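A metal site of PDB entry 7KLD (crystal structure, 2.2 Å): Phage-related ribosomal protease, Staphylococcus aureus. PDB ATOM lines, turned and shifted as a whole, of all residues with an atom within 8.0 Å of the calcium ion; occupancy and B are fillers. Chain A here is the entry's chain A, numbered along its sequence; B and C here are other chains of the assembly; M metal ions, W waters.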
ATOM      1  N   ASP A   5       9.086  31.861 -23.180  1.00  0.00           N
ATOM      2  CA  ASP A   5       8.995  30.410 -23.129  1.00  0.00           C
ATOM      3  C   ASP A   5       8.363  29.922 -24.415  1.00  0.00           C
ATOM      4  O   ASP A   5       7.199  30.218 -24.713  1.00  0.00           O
ATOM      5  CB  ASP A   5       8.160  29.946 -21.927  1.00  0.00           C
ATOM      6  CG  ASP A   5       8.865  30.158 -20.582  1.00  0.00           C
ATOM      7  OD1 ASP A   5      10.069  30.354 -20.545  1.00  0.00           O
ATOM      8  OD2 ASP A   5       8.223  30.002 -19.498  1.00  0.00           O
ATOM      9  N   ILE A   6       9.119  29.110 -25.134  1.00  0.00           N
ATOM     10  CA  ILE A   6       8.719  28.615 -26.439  1.00  0.00           C
ATOM     11  C   ILE A   6       8.655  27.103 -26.388  1.00  0.00           C
ATOM     12  O   ILE A   6       9.652  26.449 -26.050  1.00  0.00           O
ATOM     13  CB  ILE A   6       9.715  29.054 -27.522  1.00  0.00           C
ATOM     14  CG1 ILE A   6      10.021  30.541 -27.388  1.00  0.00           C
ATOM     15  CG2 ILE A   6       9.176  28.765 -28.878  1.00  0.00           C
ATOM     16  CD1 ILE A   6      11.492  30.860 -27.728  1.00  0.00           C
ATOM     17  N   ARG A 102      15.119  36.785 -21.683  1.00  0.00           N
ATOM     18  CA  ARG A 102      15.596  35.418 -21.686  1.00  0.00           C
ATOM     19  C   ARG A 102      14.694  34.685 -22.658  1.00  0.00           C
ATOM     20  O   ARG A 102      13.503  34.832 -22.609  1.00  0.00           O
ATOM     21  CB  ARG A 102      15.444  34.851 -20.303  1.00  0.00           C
ATOM     22  CG  ARG A 102      15.845  33.377 -20.147  1.00  0.00           C
ATOM     23  CD  ARG A 102      15.997  33.011 -18.669  1.00  0.00           C
ATOM     24  NE  ARG A 102      14.748  32.502 -18.076  1.00  0.00           N
ATOM     25  CZ  ARG A 102      14.527  31.232 -17.695  1.00  0.00           C
ATOM     26  NH1 ARG A 102      15.468  30.300 -17.842  1.00  0.00           N
ATOM     27  NH2 ARG A 102      13.363  30.887 -17.175  1.00  0.00           N
ATOM     28  N   LEU A 103      15.307  33.936 -23.573  1.00  0.00           N
ATOM     29  CA  LEU A 103      14.592  32.980 -24.382  1.00  0.00           C
ATOM     30  C   LEU A 103      14.807  31.577 -23.770  1.00  0.00           C
ATOM     31  O   LEU A 103      15.924  31.233 -23.389  1.00  0.00           O
ATOM     32  CB  LEU A 103      15.052  33.002 -25.829  1.00  0.00           C
ATOM     33  CG  LEU A 103      14.703  34.220 -26.699  1.00  0.00           C
ATOM     34  CD1 LEU A 103      13.214  34.451 -26.669  1.00  0.00           C
ATOM     35  CD2 LEU A 103      15.428  35.494 -26.315  1.00  0.00           C
ATOM     36  N   ASN A 104      13.749  30.799 -23.718  1.00  0.00           N
ATOM     37  CA  ASN A 104      13.785  29.449 -23.157  1.00  0.00           C
ATOM     38  C   ASN A 104      12.950  28.545 -24.033  1.00  0.00           C
ATOM     39  O   ASN A 104      11.767  28.805 -24.254  1.00  0.00           O
ATOM     40  CB  ASN A 104      13.223  29.524 -21.726  1.00  0.00           C
ATOM     41  CG  ASN A 104      13.039  28.167 -21.120  1.00  0.00           C
ATOM     42  OD1 ASN A 104      13.959  27.354 -21.133  1.00  0.00           O
ATOM     43  ND2 ASN A 104      11.784  27.863 -20.678  1.00  0.00           N
ATOM     44  N   TYR A 105      13.552  27.478 -24.554  1.00  0.00           N
ATOM     45  CA  TYR A 105      12.846  26.368 -25.221  1.00  0.00           C
ATOM     46  C   TYR A 105      12.393  25.257 -24.240  1.00  0.00           C
ATOM     47  O   TYR A 105      13.165  24.826 -23.375  1.00  0.00           O
ATOM     48  CB  TYR A 105      13.691  25.797 -26.348  1.00  0.00           C
ATOM     49  CG  TYR A 105      13.815  26.754 -27.501  1.00  0.00           C
ATOM     50  CD1 TYR A 105      14.721  27.830 -27.458  1.00  0.00           C
ATOM     51  CD2 TYR A 105      13.014  26.633 -28.612  1.00  0.00           C
ATOM     52  CE1 TYR A 105      14.784  28.753 -28.477  1.00  0.00           C
ATOM     53  CE2 TYR A 105      13.133  27.505 -29.666  1.00  0.00           C
ATOM     54  CZ  TYR A 105      14.012  28.557 -29.589  1.00  0.00           C
ATOM     55  OH  TYR A 105      14.075  29.466 -30.637  1.00  0.00           O
ATOM     56  N   LYS A 106      11.174  24.789 -24.426  1.00  0.00           N
ATOM     57  CA  LYS A 106      10.675  23.622 -23.722  1.00  0.00           C
ATOM     58  C   LYS A 106      10.203  22.611 -24.743  1.00  0.00           C
ATOM     59  O   LYS A 106       9.475  21.696 -24.377  1.00  0.00           O
ATOM     60  CB  LYS A 106       9.553  23.987 -22.785  1.00  0.00           C
ATOM     61  CG  LYS A 106       9.665  25.394 -22.223  1.00  0.00           C
ATOM     62  CD  LYS A 106       8.776  25.592 -20.999  1.00  0.00           C
ATOM     63  CE  LYS A 106       7.307  25.518 -21.354  1.00  0.00           C
ATOM     64  NZ  LYS A 106       6.488  24.991 -20.179  1.00  0.00           N
ATOM     65  OXT LYS A 106      10.548  22.694 -25.931  1.00  0.00           O
ATOM     66  N   ASN B   9      23.306  27.300 -23.354  1.00  0.00           N
ATOM     67  CA  ASN B   9      21.951  27.469 -22.863  1.00  0.00           C
ATOM     68  C   ASN B   9      21.020  27.783 -24.056  1.00  0.00           C
ATOM     69  O   ASN B   9      21.472  27.749 -25.221  1.00  0.00           O
ATOM     70  CB  ASN B   9      21.893  28.508 -21.724  1.00  0.00           C
ATOM     71  CG  ASN B   9      22.102  29.946 -22.199  1.00  0.00           C
ATOM     72  OD1 ASN B   9      22.184  30.231 -23.395  1.00  0.00           O
ATOM     73  ND2 ASN B   9      22.139  30.872 -21.223  1.00  0.00           N
ATOM     74  N   ASP B  10      19.741  28.072 -23.770  1.00  0.00           N
ATOM     75  CA  ASP B  10      18.908  28.168 -24.962  1.00  0.00           C
ATOM     76  C   ASP B  10      19.041  29.512 -25.692  1.00  0.00           C
ATOM     77  O   ASP B  10      18.808  29.567 -26.915  1.00  0.00           O
ATOM     78  CB  ASP B  10      17.413  27.882 -24.622  1.00  0.00           C
ATOM     79  CG  ASP B  10      17.156  26.432 -24.211  1.00  0.00           C
ATOM     80  OD1 ASP B  10      16.250  26.221 -23.382  1.00  0.00           O
ATOM     81  OD2 ASP B  10      17.849  25.516 -24.715  1.00  0.00           O
ATOM     82  N   GLU B  11      19.741  30.515 -25.117  1.00  0.00           N
ATOM     83  CA  GLU B  11      20.106  31.761 -25.808  1.00  0.00           C
ATOM     84  C   GLU B  11      21.435  31.708 -26.546  1.00  0.00           C
ATOM     85  O   GLU B  11      21.900  32.710 -27.053  1.00  0.00           O
ATOM     86  CB  GLU B  11      20.156  32.916 -24.803  1.00  0.00           C
ATOM     87  CG  GLU B  11      18.839  33.155 -24.047  1.00  0.00           C
ATOM     88  CD  GLU B  11      18.892  34.429 -23.240  1.00  0.00           C
ATOM     89  OE1 GLU B  11      19.925  34.719 -22.654  1.00  0.00           O
ATOM     90  OE2 GLU B  11      17.935  35.203 -23.218  1.00  0.00           O
ATOM     91  N   LYS B 106      25.984  20.547 -25.901  1.00  0.00           N
ATOM     92  CA  LYS B 106      24.982  20.363 -24.904  1.00  0.00           C
ATOM     93  C   LYS B 106      25.040  19.030 -24.261  1.00  0.00           C
ATOM     94  O   LYS B 106      24.315  18.148 -24.502  1.00  0.00           O
ATOM     95  CB  LYS B 106      23.600  20.722 -25.421  1.00  0.00           C
ATOM     96  CG  LYS B 106      23.254  22.112 -25.022  1.00  0.00           C
ATOM     97  CD  LYS B 106      21.802  22.522 -25.359  1.00  0.00           C
ATOM     98  CE  LYS B 106      20.948  22.759 -24.145  1.00  0.00           C
ATOM     99  NZ  LYS B 106      21.733  23.192 -22.950  1.00  0.00           N
ATOM    100  OXT LYS B 106      25.814  18.826 -23.392  1.00  0.00           O
ATOM    101  N   LYS C 106       6.653  19.037 -18.193  1.00  0.00           N
ATOM    102  CA  LYS C 106       7.780  19.676 -18.788  1.00  0.00           C
ATOM    103  C   LYS C 106       7.501  20.202 -20.145  1.00  0.00           C
ATOM    104  O   LYS C 106       7.843  19.689 -21.135  1.00  0.00           O
ATOM    105  CB  LYS C 106       9.021  18.803 -18.724  1.00  0.00           C
ATOM    106  CG  LYS C 106       9.854  19.190 -17.555  1.00  0.00           C
ATOM    107  CD  LYS C 106      11.222  18.471 -17.490  1.00  0.00           C
ATOM    108  CE  LYS C 106      12.393  19.394 -17.680  1.00  0.00           C
ATOM    109  NZ  LYS C 106      12.112  20.797 -17.253  1.00  0.00           N
ATOM    110  OXT LYS C 106       6.956  21.242 -20.274  1.00  0.00           O
HETATM  111 CA    CA M   1      15.149  24.986 -21.844  1.00  0.00          CA
HETATM  112  O   HOH W   1      12.758  24.634 -19.392  1.00  0.00           O
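N of Ile 6 lies within hydrogen-bond range of O of Asn 104, 2.8 Å away.
The side-chain amide nitrogen of Asn 104 sits at hydrogen-bond distance from the side-chain carboxylate of Asp 5, at 3.0 Å.
Three residues have an atom within 4 Å of the calcium ion: Asn 104, Tyr 105 and Asp 10 of chain B.
The nearest printed residue that does not touch the calcium ion is Lys 106 of chain A (4.7 Å).
The calcium ion is bound by the side-chain carboxylate (OD1) of Asp 10 of chain B, the backbone carbonyl oxygen (O) of Tyr 105 and the side-chain amide oxygen (OD1) of Asn 104.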
